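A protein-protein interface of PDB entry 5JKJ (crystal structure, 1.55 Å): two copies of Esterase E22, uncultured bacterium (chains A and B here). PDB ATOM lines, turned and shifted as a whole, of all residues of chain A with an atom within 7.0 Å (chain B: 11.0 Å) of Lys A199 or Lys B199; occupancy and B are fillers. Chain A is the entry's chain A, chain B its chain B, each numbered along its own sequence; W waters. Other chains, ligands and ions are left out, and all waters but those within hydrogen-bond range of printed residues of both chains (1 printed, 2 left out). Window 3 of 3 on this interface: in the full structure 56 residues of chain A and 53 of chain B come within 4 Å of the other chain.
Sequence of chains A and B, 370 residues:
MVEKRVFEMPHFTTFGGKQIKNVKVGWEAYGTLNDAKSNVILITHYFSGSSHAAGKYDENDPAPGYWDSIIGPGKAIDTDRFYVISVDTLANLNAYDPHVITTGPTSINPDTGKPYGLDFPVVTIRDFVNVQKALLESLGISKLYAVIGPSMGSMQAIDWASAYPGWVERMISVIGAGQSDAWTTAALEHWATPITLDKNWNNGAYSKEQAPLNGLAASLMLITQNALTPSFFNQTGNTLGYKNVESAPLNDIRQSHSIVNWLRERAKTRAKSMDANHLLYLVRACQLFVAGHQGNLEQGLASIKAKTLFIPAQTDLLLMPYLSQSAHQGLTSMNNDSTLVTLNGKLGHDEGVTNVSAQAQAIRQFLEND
O of Leu A197 sits close to O of Leu B197 (3.1 Å).
N of Asn A200 sits at hydrogen-bond distance from OD1 of Asp A198, at 2.9 Å.
OD2 of Asp B198 lies within hydrogen-bond range of N of Asn B214, 3.3 Å away.
The backbone NH (N) of Gly B215 is in hydrogen-bond range of the side-chain carboxylate (OD2) of Asp B198.
Among the printed residues, merely in contact across the chains: Pro A194 with Leu B197 (3.5 Å), Leu A197 with Pro B194 (3.5 Å), Leu A197 with Asn B214 (3.8 Å), Leu A197 with Gly B215 (3.8 Å), Leu A197 with Ala B218 (3.9 Å), Asp A198 with Leu B197 (3.9 Å) and Lys A199 with Lys B199 (3.9 Å).
Lys A199 touches just one residue of chain B: Lys B199.
Of the printed residues of chain A, Lys B199 touches Lys A199.
No residue of chain B comes within 4 Å of Asn A200.
Asn A202 touches none of the printed residues of chain B.
Of the printed residues of chain A, Asn B214 touches Leu A197 (3.8 Å).
Of the printed residues of chain B, Leu A197 touches Pro B194 (3.5 Å), Leu B197 (3.1 Å), Asn B214 (3.8 Å), Gly B215 (3.8 Å) and Ala B218 (3.9 Å).
Of the printed residues of chain B, Pro A194 touches Leu B197.
Printed residues of chain A within 4 Å of Pro B194: Leu A197 (3.5 Å).
Of the printed residues of chain A, Gly B215 touches Leu A197.
Of the 25 printed residues of chain B, 6 touch a printed residue of chain A.
Among the printed residues, 8 pairs touch across the chains.
Among the printed residues, no Asp or Glu carboxylate lies within 4 Å of a Lys or Arg side-chain nitrogen of the other chain.
Pro A194 touches Leu B197, and with the chains exchanged Leu A197 touches Pro B194.
Leu B197 touches its own counterpart, Leu A197.
Asp A198 touches Leu B197, but with the chains exchanged Leu A197 does not touch Asp B198 (4.4 Å).
Lys B199 touches its own counterpart, Lys A199.
Of the 8 pairs that touch across the chains among the printed residues, 4 have their exchanged pair printed and touching as well.
Water W1 bridges the backbone carbonyl oxygen of Leu A197 and the backbone NH of Lys B199.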
ATOM      1  N   PRO A 194      21.960  17.156  14.447  1.00  0.00           N
ATOM      2  CA  PRO A 194      23.381  16.931  14.785  1.00  0.00           C
ATOM      3  C   PRO A 194      24.091  18.196  15.229  1.00  0.00           C
ATOM      4  O   PRO A 194      24.937  18.149  16.133  1.00  0.00           O
ATOM      5  CB  PRO A 194      23.962  16.358  13.484  1.00  0.00           C
ATOM      6  CG  PRO A 194      22.763  15.710  12.796  1.00  0.00           C
ATOM      7  CD  PRO A 194      21.639  16.662  13.093  1.00  0.00           C
ATOM      8  N   ILE A 195      23.743  19.337  14.629  1.00  0.00           N
ATOM      9  CA  ILE A 195      24.331  20.613  15.023  1.00  0.00           C
ATOM     10  C   ILE A 195      23.958  20.953  16.460  1.00  0.00           C
ATOM     11  O   ILE A 195      24.814  21.344  17.260  1.00  0.00           O
ATOM     12  CB  ILE A 195      23.894  21.722  14.048  1.00  0.00           C
ATOM     13  CG1 ILE A 195      24.628  21.548  12.716  1.00  0.00           C
ATOM     14  CG2 ILE A 195      24.173  23.119  14.643  1.00  0.00           C
ATOM     15  CD1 ILE A 195      23.886  22.171  11.540  1.00  0.00           C
ATOM     16  N   THR A 196      22.673  20.816  16.806  1.00  0.00           N
ATOM     17  CA  THR A 196      22.235  21.205  18.144  1.00  0.00           C
ATOM     18  C   THR A 196      22.720  20.236  19.211  1.00  0.00           C
ATOM     19  O   THR A 196      22.755  20.606  20.389  1.00  0.00           O
ATOM     20  CB  THR A 196      20.709  21.338  18.209  1.00  0.00           C
ATOM     21  OG1 THR A 196      20.088  20.066  17.994  1.00  0.00           O
ATOM     22  CG2 THR A 196      20.214  22.358  17.179  1.00  0.00           C
ATOM     23  N   LEU A 197      23.114  19.019  18.829  1.00  0.00           N
ATOM     24  CA  LEU A 197      23.700  18.093  19.792  1.00  0.00           C
ATOM     25  C   LEU A 197      25.153  18.418  20.112  1.00  0.00           C
ATOM     26  O   LEU A 197      25.605  18.163  21.237  1.00  0.00           O
ATOM     27  CB  LEU A 197      23.598  16.660  19.261  1.00  0.00           C
ATOM     28  CG  LEU A 197      22.200  16.056  19.251  1.00  0.00           C
ATOM     29  CD1 LEU A 197      22.175  14.778  18.431  1.00  0.00           C
ATOM     30  CD2 LEU A 197      21.759  15.770  20.688  1.00  0.00           C
ATOM     31  N   ASP A 198      25.903  18.937  19.138  1.00  0.00           N
ATOM     32  CA  ASP A 198      27.322  19.229  19.301  1.00  0.00           C
ATOM     33  C   ASP A 198      27.523  20.264  20.405  1.00  0.00           C
ATOM     34  O   ASP A 198      26.998  21.374  20.322  1.00  0.00           O
ATOM     35  CB  ASP A 198      27.854  19.717  17.949  1.00  0.00           C
ATOM     36  CG  ASP A 198      29.347  19.966  17.921  1.00  0.00           C
ATOM     37  OD1 ASP A 198      29.957  20.314  18.955  1.00  0.00           O
ATOM     38  OD2 ASP A 198      29.916  19.851  16.818  1.00  0.00           O
ATOM     39  N   LYS A 199      28.297  19.897  21.437  1.00  0.00           N
ATOM     40  CA  LYS A 199      28.482  20.783  22.585  1.00  0.00           C
ATOM     41  C   LYS A 199      29.003  22.152  22.171  1.00  0.00           C
ATOM     42  O   LYS A 199      28.661  23.161  22.797  1.00  0.00           O
ATOM     43  CB  LYS A 199      29.432  20.137  23.599  1.00  0.00           C
ATOM     44  CG  LYS A 199      29.613  20.932  24.884  1.00  0.00           C
ATOM     45  CD  LYS A 199      30.721  20.333  25.746  1.00  0.00           C
ATOM     46  CE  LYS A 199      30.931  21.142  27.015  1.00  0.00           C
ATOM     47  NZ  LYS A 199      29.681  21.207  27.817  1.00  0.00           N
ATOM     48  N   ASN A 200      29.808  22.213  21.110  1.00  0.00           N
ATOM     49  CA  ASN A 200      30.360  23.486  20.673  1.00  0.00           C
ATOM     50  C   ASN A 200      29.288  24.441  20.166  1.00  0.00           C
ATOM     51  O   ASN A 200      29.563  25.635  20.012  1.00  0.00           O
ATOM     52  CB  ASN A 200      31.394  23.254  19.570  1.00  0.00           C
ATOM     53  CG  ASN A 200      32.572  22.420  20.033  1.00  0.00           C
ATOM     54  OD1 ASN A 200      32.642  21.213  19.780  1.00  0.00           O
ATOM     55  ND2 ASN A 200      33.505  23.058  20.701  1.00  0.00           N
ATOM     56  N   TRP A 201      28.085  23.944  19.883  1.00  0.00           N
ATOM     57  CA  TRP A 201      27.048  24.826  19.363  1.00  0.00           C
ATOM     58  C   TRP A 201      26.733  25.937  20.355  1.00  0.00           C
ATOM     59  O   TRP A 201      26.490  27.087  19.961  1.00  0.00           O
ATOM     60  CB  TRP A 201      25.796  24.009  19.030  1.00  0.00           C
ATOM     61  CG  TRP A 201      24.695  24.844  18.409  1.00  0.00           C
ATOM     62  CD1 TRP A 201      24.799  25.661  17.315  1.00  0.00           C
ATOM     63  CD2 TRP A 201      23.338  24.934  18.854  1.00  0.00           C
ATOM     64  NE1 TRP A 201      23.580  26.255  17.056  1.00  0.00           N
ATOM     65  CE2 TRP A 201      22.668  25.820  17.982  1.00  0.00           C
ATOM     66  CE3 TRP A 201      22.620  24.349  19.905  1.00  0.00           C
ATOM     67  CZ2 TRP A 201      21.313  26.136  18.131  1.00  0.00           C
ATOM     68  CZ3 TRP A 201      21.271  24.666  20.051  1.00  0.00           C
ATOM     69  CH2 TRP A 201      20.636  25.553  19.165  1.00  0.00           C
ATOM     70  N   ASN A 202      26.750  25.622  21.649  1.00  0.00           N
ATOM     71  CA  ASN A 202      26.578  26.625  22.699  1.00  0.00           C
ATOM     72  C   ASN A 202      25.304  27.436  22.477  1.00  0.00           C
ATOM     73  O   ASN A 202      25.306  28.666  22.561  1.00  0.00           O
ATOM     74  CB  ASN A 202      27.797  27.547  22.784  1.00  0.00           C
ATOM     75  CG  ASN A 202      27.865  28.300  24.098  1.00  0.00           C
ATOM     76  OD1 ASN A 202      27.392  27.815  25.131  1.00  0.00           O
ATOM     77  ND2 ASN A 202      28.445  29.495  24.065  1.00  0.00           N
ATOM     78  N   ASN A 203      24.211  26.737  22.158  1.00  0.00           N
ATOM     79  CA  ASN A 203      22.901  27.362  21.969  1.00  0.00           C
ATOM     80  C   ASN A 203      22.947  28.460  20.907  1.00  0.00           C
ATOM     81  O   ASN A 203      22.180  29.428  20.957  1.00  0.00           O
ATOM     82  CB  ASN A 203      22.363  27.905  23.301  1.00  0.00           C
ATOM     83  CG  ASN A 203      20.856  28.116  23.294  1.00  0.00           C
ATOM     84  OD1 ASN A 203      20.136  27.558  22.460  1.00  0.00           O
ATOM     85  ND2 ASN A 203      20.370  28.919  24.239  1.00  0.00           N
ATOM     86  N   GLN A 210      35.590  28.220  16.891  1.00  0.00           N
ATOM     87  CA  GLN A 210      35.122  27.243  17.868  1.00  0.00           C
ATOM     88  C   GLN A 210      33.761  26.688  17.459  1.00  0.00           C
ATOM     89  O   GLN A 210      32.908  26.381  18.296  1.00  0.00           O
ATOM     90  CB  GLN A 210      35.075  27.854  19.260  1.00  0.00           C
ATOM     91  CG  GLN A 210      36.442  28.370  19.704  1.00  0.00           C
ATOM     92  CD  GLN A 210      36.425  28.967  21.093  1.00  0.00           C
ATOM     93  OE1 GLN A 210      35.368  29.293  21.632  1.00  0.00           O
ATOM     94  NE2 GLN A 210      37.607  29.109  21.686  1.00  0.00           N
ATOM     95  N   PRO A 212      30.678  24.280  15.848  1.00  0.00           N
ATOM     96  CA  PRO A 212      30.317  22.859  15.967  1.00  0.00           C
ATOM     97  C   PRO A 212      30.635  22.090  14.690  1.00  0.00           C
ATOM     98  O   PRO A 212      29.739  21.675  13.940  1.00  0.00           O
ATOM     99  CB  PRO A 212      28.808  22.910  16.252  1.00  0.00           C
ATOM    100  CG  PRO A 212      28.356  24.158  15.553  1.00  0.00           C
ATOM    101  CD  PRO A 212      29.486  25.146  15.765  1.00  0.00           C
ATOM    102  N   ALA B 192      24.028   6.385  14.004  1.00  0.00           N
ATOM    103  CA  ALA B 192      25.077   6.396  15.016  1.00  0.00           C
ATOM    104  C   ALA B 192      25.558   7.801  15.348  1.00  0.00           C
ATOM    105  O   ALA B 192      25.852   8.094  16.517  1.00  0.00           O
ATOM    106  CB  ALA B 192      26.266   5.549  14.548  1.00  0.00           C
ATOM    107  N   THR B 193      25.662   8.681  14.350  1.00  0.00           N
ATOM    108  CA  THR B 193      26.341   9.949  14.596  1.00  0.00           C
ATOM    109  C   THR B 193      25.676  10.808  15.672  1.00  0.00           C
ATOM    110  O   THR B 193      26.416  11.445  16.446  1.00  0.00           O
ATOM    111  CB  THR B 193      26.504  10.726  13.288  1.00  0.00           C
ATOM    112  OG1 THR B 193      27.164   9.892  12.324  1.00  0.00           O
ATOM    113  CG2 THR B 193      27.389  11.882  13.535  1.00  0.00           C
ATOM    114  N   PRO B 194      24.344  10.856  15.822  1.00  0.00           N
ATOM    115  CA  PRO B 194      23.789  11.711  16.890  1.00  0.00           C
ATOM    116  C   PRO B 194      24.233  11.307  18.286  1.00  0.00           C
ATOM    117  O   PRO B 194      24.440  12.178  19.136  1.00  0.00           O
ATOM    118  CB  PRO B 194      22.271  11.568  16.702  1.00  0.00           C
ATOM    119  CG  PRO B 194      22.127  11.206  15.261  1.00  0.00           C
ATOM    120  CD  PRO B 194      23.262  10.264  15.013  1.00  0.00           C
ATOM    121  N   ILE B 195      24.377  10.006  18.545  1.00  0.00           N
ATOM    122  CA  ILE B 195      24.871   9.554  19.845  1.00  0.00           C
ATOM    123  C   ILE B 195      26.309  10.019  20.060  1.00  0.00           C
ATOM    124  O   ILE B 195      26.670  10.481  21.153  1.00  0.00           O
ATOM    125  CB  ILE B 195      24.729   8.025  19.947  1.00  0.00           C
ATOM    126  CG1 ILE B 195      23.245   7.655  20.065  1.00  0.00           C
ATOM    127  CG2 ILE B 195      25.543   7.481  21.108  1.00  0.00           C
ATOM    128  CD1 ILE B 195      22.930   6.228  19.665  1.00  0.00           C
ATOM    129  N   THR B 196      27.141   9.953  19.016  1.00  0.00           N
ATOM    130  CA  THR B 196      28.541  10.337  19.175  1.00  0.00           C
ATOM    131  C   THR B 196      28.696  11.830  19.402  1.00  0.00           C
ATOM    132  O   THR B 196      29.735  12.262  19.914  1.00  0.00           O
ATOM    133  CB  THR B 196      29.387   9.925  17.964  1.00  0.00           C
ATOM    134  OG1 THR B 196      29.028  10.708  16.820  1.00  0.00           O
ATOM    135  CG2 THR B 196      29.229   8.451  17.656  1.00  0.00           C
ATOM    136  N   LEU B 197      27.671  12.621  19.067  1.00  0.00           N
ATOM    137  CA  LEU B 197      27.711  14.064  19.245  1.00  0.00           C
ATOM    138  C   LEU B 197      27.180  14.522  20.592  1.00  0.00           C
ATOM    139  O   LEU B 197      27.418  15.676  20.964  1.00  0.00           O
ATOM    140  CB  LEU B 197      26.895  14.749  18.146  1.00  0.00           C
ATOM    141  CG  LEU B 197      27.568  14.672  16.784  1.00  0.00           C
ATOM    142  CD1 LEU B 197      26.543  15.020  15.718  1.00  0.00           C
ATOM    143  CD2 LEU B 197      28.766  15.617  16.736  1.00  0.00           C
ATOM    144  N   ASP B 198      26.469  13.660  21.313  1.00  0.00           N
ATOM    145  CA  ASP B 198      25.871  14.034  22.588  1.00  0.00           C
ATOM    146  C   ASP B 198      26.965  14.178  23.638  1.00  0.00           C
ATOM    147  O   ASP B 198      27.753  13.254  23.846  1.00  0.00           O
ATOM    148  CB  ASP B 198      24.853  12.962  22.986  1.00  0.00           C
ATOM    149  CG  ASP B 198      24.073  13.293  24.254  1.00  0.00           C
ATOM    150  OD1 ASP B 198      24.670  13.685  25.274  1.00  0.00           O
ATOM    151  OD2 ASP B 198      22.840  13.117  24.250  1.00  0.00           O
ATOM    152  N   LYS B 199      27.005  15.346  24.301  1.00  0.00           N
ATOM    153  CA  LYS B 199      28.065  15.645  25.268  1.00  0.00           C
ATOM    154  C   LYS B 199      28.137  14.645  26.416  1.00  0.00           C
ATOM    155  O   LYS B 199      29.184  14.542  27.061  1.00  0.00           O
ATOM    156  CB  LYS B 199      27.877  17.054  25.842  1.00  0.00           C
ATOM    157  CG  LYS B 199      26.620  17.223  26.690  1.00  0.00           C
ATOM    158  CD  LYS B 199      26.369  18.688  26.991  1.00  0.00           C
ATOM    159  CE  LYS B 199      26.143  18.941  28.465  1.00  0.00           C
ATOM    160  NZ  LYS B 199      25.995  20.406  28.723  1.00  0.00           N
ATOM    161  N   ASN B 200      27.059  13.917  26.701  1.00  0.00           N
ATOM    162  CA  ASN B 200      27.089  12.931  27.775  1.00  0.00           C
ATOM    163  C   ASN B 200      27.622  11.578  27.328  1.00  0.00           C
ATOM    164  O   ASN B 200      27.823  10.704  28.178  1.00  0.00           O
ATOM    165  CB  ASN B 200      25.692  12.738  28.377  1.00  0.00           C
ATOM    166  CG  ASN B 200      25.316  13.835  29.364  1.00  0.00           C
ATOM    167  OD1 ASN B 200      26.091  14.761  29.622  1.00  0.00           O
ATOM    168  ND2 ASN B 200      24.114  13.734  29.919  1.00  0.00           N
ATOM    169  N   TRP B 201      27.839  11.366  26.025  1.00  0.00           N
ATOM    170  CA  TRP B 201      28.284  10.049  25.579  1.00  0.00           C
ATOM    171  C   TRP B 201      29.630   9.685  26.192  1.00  0.00           C
ATOM    172  O   TRP B 201      29.845   8.535  26.587  1.00  0.00           O
ATOM    173  CB  TRP B 201      28.346  10.007  24.051  1.00  0.00           C
ATOM    174  CG  TRP B 201      28.716   8.670  23.484  1.00  0.00           C
ATOM    175  CD1 TRP B 201      28.130   7.468  23.753  1.00  0.00           C
ATOM    176  CD2 TRP B 201      29.725   8.415  22.503  1.00  0.00           C
ATOM    177  NE1 TRP B 201      28.736   6.474  23.023  1.00  0.00           N
ATOM    178  CE2 TRP B 201      29.725   7.028  22.249  1.00  0.00           C
ATOM    179  CE3 TRP B 201      30.652   9.222  21.835  1.00  0.00           C
ATOM    180  CZ2 TRP B 201      30.601   6.433  21.343  1.00  0.00           C
ATOM    181  CZ3 TRP B 201      31.516   8.635  20.934  1.00  0.00           C
ATOM    182  CH2 TRP B 201      31.487   7.248  20.697  1.00  0.00           C
ATOM    183  N   ASN B 202      30.536  10.661  26.309  1.00  0.00           N
ATOM    184  CA  ASN B 202      31.846  10.434  26.924  1.00  0.00           C
ATOM    185  C   ASN B 202      32.544   9.223  26.309  1.00  0.00           C
ATOM    186  O   ASN B 202      33.093   8.363  27.007  1.00  0.00           O
ATOM    187  CB  ASN B 202      31.721  10.285  28.442  1.00  0.00           C
ATOM    188  CG  ASN B 202      33.054  10.431  29.146  1.00  0.00           C
ATOM    189  OD1 ASN B 202      33.934  11.163  28.685  1.00  0.00           O
ATOM    190  ND2 ASN B 202      33.224   9.713  30.251  1.00  0.00           N
ATOM    191  N   ASN B 203      32.504   9.145  24.980  1.00  0.00           N
ATOM    192  CA  ASN B 203      33.172   8.077  24.236  1.00  0.00           C
ATOM    193  C   ASN B 203      32.747   6.692  24.710  1.00  0.00           C
ATOM    194  O   ASN B 203      33.526   5.732  24.660  1.00  0.00           O
ATOM    195  CB  ASN B 203      34.686   8.247  24.312  1.00  0.00           C
ATOM    196  CG  ASN B 203      35.156   9.350  23.416  1.00  0.00           C
ATOM    197  OD1 ASN B 203      34.944   9.297  22.203  1.00  0.00           O
ATOM    198  ND2 ASN B 203      35.753  10.386  23.999  1.00  0.00           N
ATOM    199  N   GLY B 204      31.508   6.586  25.180  1.00  0.00           N
ATOM    200  CA  GLY B 204      30.927   5.316  25.554  1.00  0.00           C
ATOM    201  C   GLY B 204      30.953   5.018  27.036  1.00  0.00           C
ATOM    202  O   GLY B 204      30.315   4.047  27.463  1.00  0.00           O
ATOM    203  N   ALA B 205      31.642   5.839  27.835  1.00  0.00           N
ATOM    204  CA  ALA B 205      31.869   5.542  29.245  1.00  0.00           C
ATOM    205  C   ALA B 205      30.824   6.152  30.179  1.00  0.00           C
ATOM    206  O   ALA B 205      31.084   6.275  31.383  1.00  0.00           O
ATOM    207  CB  ALA B 205      33.269   6.010  29.654  1.00  0.00           C
ATOM    208  N   TYR B 206      29.648   6.502  29.673  1.00  0.00           N
ATOM    209  CA  TYR B 206      28.645   7.181  30.482  1.00  0.00           C
ATOM    210  C   TYR B 206      28.029   6.253  31.527  1.00  0.00           C
ATOM    211  O   TYR B 206      27.970   5.032  31.362  1.00  0.00           O
ATOM    212  CB  TYR B 206      27.546   7.741  29.586  1.00  0.00           C
ATOM    213  CG  TYR B 206      26.888   6.690  28.735  1.00  0.00           C
ATOM    214  CD1 TYR B 206      25.796   5.970  29.205  1.00  0.00           C
ATOM    215  CD2 TYR B 206      27.342   6.432  27.450  1.00  0.00           C
ATOM    216  CE1 TYR B 206      25.182   4.998  28.419  1.00  0.00           C
ATOM    217  CE2 TYR B 206      26.741   5.451  26.663  1.00  0.00           C
ATOM    218  CZ  TYR B 206      25.665   4.747  27.149  1.00  0.00           C
ATOM    219  OH  TYR B 206      25.065   3.792  26.353  1.00  0.00           O
ATOM    220  N   SER B 207      27.557   6.853  32.613  1.00  0.00           N
ATOM    221  CA  SER B 207      26.745   6.135  33.581  1.00  0.00           C
ATOM    222  C   SER B 207      25.285   6.155  33.149  1.00  0.00           C
ATOM    223  O   SER B 207      24.843   7.029  32.398  1.00  0.00           O
ATOM    224  CB  SER B 207      26.889   6.748  34.975  1.00  0.00           C
ATOM    225  OG  SER B 207      26.283   8.026  35.025  1.00  0.00           O
ATOM    226  N   GLN B 210      23.560   9.471  33.710  1.00  0.00           N
ATOM    227  CA  GLN B 210      23.989  10.591  32.879  1.00  0.00           C
ATOM    228  C   GLN B 210      24.174  10.119  31.449  1.00  0.00           C
ATOM    229  O   GLN B 210      25.193  10.361  30.801  1.00  0.00           O
ATOM    230  CB  GLN B 210      25.272  11.217  33.423  1.00  0.00           C
ATOM    231  CG  GLN B 210      25.072  11.910  34.762  1.00  0.00           C
ATOM    232  CD  GLN B 210      26.256  11.743  35.688  1.00  0.00           C
ATOM    233  OE1 GLN B 210      26.659  12.685  36.374  1.00  0.00           O
ATOM    234  NE2 GLN B 210      26.818  10.530  35.721  1.00  0.00           N
ATOM    235  N   ALA B 211      23.165   9.414  30.946  1.00  0.00           N
ATOM    236  CA  ALA B 211      23.228   8.828  29.620  1.00  0.00           C
ATOM    237  C   ALA B 211      23.037   9.898  28.548  1.00  0.00           C
ATOM    238  O   ALA B 211      22.513  10.980  28.815  1.00  0.00           O
ATOM    239  CB  ALA B 211      22.165   7.735  29.482  1.00  0.00           C
ATOM    240  N   PRO B 212      23.486   9.619  27.312  1.00  0.00           N
ATOM    241  CA  PRO B 212      23.257  10.538  26.178  1.00  0.00           C
ATOM    242  C   PRO B 212      21.831  10.416  25.653  1.00  0.00           C
ATOM    243  O   PRO B 212      21.563   9.915  24.556  1.00  0.00           O
ATOM    244  CB  PRO B 212      24.309  10.073  25.168  1.00  0.00           C
ATOM    245  CG  PRO B 212      24.431   8.617  25.433  1.00  0.00           C
ATOM    246  CD  PRO B 212      24.382   8.509  26.944  1.00  0.00           C
ATOM    247  N   LEU B 213      20.881  10.880  26.470  1.00  0.00           N
ATOM    248  CA  LEU B 213      19.469  10.678  26.161  1.00  0.00           C
ATOM    249  C   LEU B 213      19.040  11.480  24.937  1.00  0.00           C
ATOM    250  O   LEU B 213      18.213  11.011  24.145  1.00  0.00           O
ATOM    251  CB  LEU B 213      18.608  11.046  27.368  1.00  0.00           C
ATOM    252  CG  LEU B 213      18.876  10.286  28.667  1.00  0.00           C
ATOM    253  CD1 LEU B 213      17.920  10.788  29.735  1.00  0.00           C
ATOM    254  CD2 LEU B 213      18.746   8.776  28.481  1.00  0.00           C
ATOM    255  N   ASN B 214      19.590  12.680  24.756  1.00  0.00           N
ATOM    256  CA  ASN B 214      19.188  13.493  23.612  1.00  0.00           C
ATOM    257  C   ASN B 214      19.707  12.904  22.308  1.00  0.00           C
ATOM    258  O   ASN B 214      18.996  12.899  21.296  1.00  0.00           O
ATOM    259  CB  ASN B 214      19.675  14.934  23.786  1.00  0.00           C
ATOM    260  CG  ASN B 214      18.840  15.717  24.779  1.00  0.00           C
ATOM    261  OD1 ASN B 214      17.618  15.575  24.834  1.00  0.00           O
ATOM    262  ND2 ASN B 214      19.501  16.544  25.574  1.00  0.00           N
ATOM    263  N   GLY B 215      20.944  12.406  22.312  1.00  0.00           N
ATOM    264  CA  GLY B 215      21.478  11.792  21.114  1.00  0.00           C
ATOM    265  C   GLY B 215      20.745  10.512  20.781  1.00  0.00           C
ATOM    266  O   GLY B 215      20.443  10.248  19.614  1.00  0.00           O
ATOM    267  N   LEU B 216      20.443   9.706  21.804  1.00  0.00           N
ATOM    268  CA  LEU B 216      19.673   8.485  21.591  1.00  0.00           C
ATOM    269  C   LEU B 216      18.286   8.789  21.035  1.00  0.00           C
ATOM    270  O   LEU B 216      17.828   8.113  20.104  1.00  0.00           O
ATOM    271  CB  LEU B 216      19.573   7.701  22.902  1.00  0.00           C
ATOM    272  CG  LEU B 216      18.756   6.412  22.819  1.00  0.00           C
ATOM    273  CD1 LEU B 216      19.308   5.484  21.752  1.00  0.00           C
ATOM    274  CD2 LEU B 216      18.772   5.748  24.187  1.00  0.00           C
ATOM    275  N   ALA B 218      17.465  11.435  19.288  1.00  0.00           N
ATOM    276  CA  ALA B 218      17.679  11.872  17.906  1.00  0.00           C
ATOM    277  C   ALA B 218      17.872  10.688  16.965  1.00  0.00           C
ATOM    278  O   ALA B 218      17.299  10.652  15.871  1.00  0.00           O
ATOM    279  CB  ALA B 218      18.885  12.809  17.835  1.00  0.00           C
ATOM    280  N   ALA B 276      22.251   3.534  24.318  1.00  0.00           N
ATOM    281  CA  ALA B 276      22.878   4.203  23.186  1.00  0.00           C
ATOM    282  C   ALA B 276      24.054   3.406  22.615  1.00  0.00           C
ATOM    283  O   ALA B 276      24.162   3.249  21.394  1.00  0.00           O
ATOM    284  CB  ALA B 276      23.318   5.609  23.602  1.00  0.00           C
HETATM  285  O   HOH W   1      25.086  17.454  23.641  1.00  0.00           O
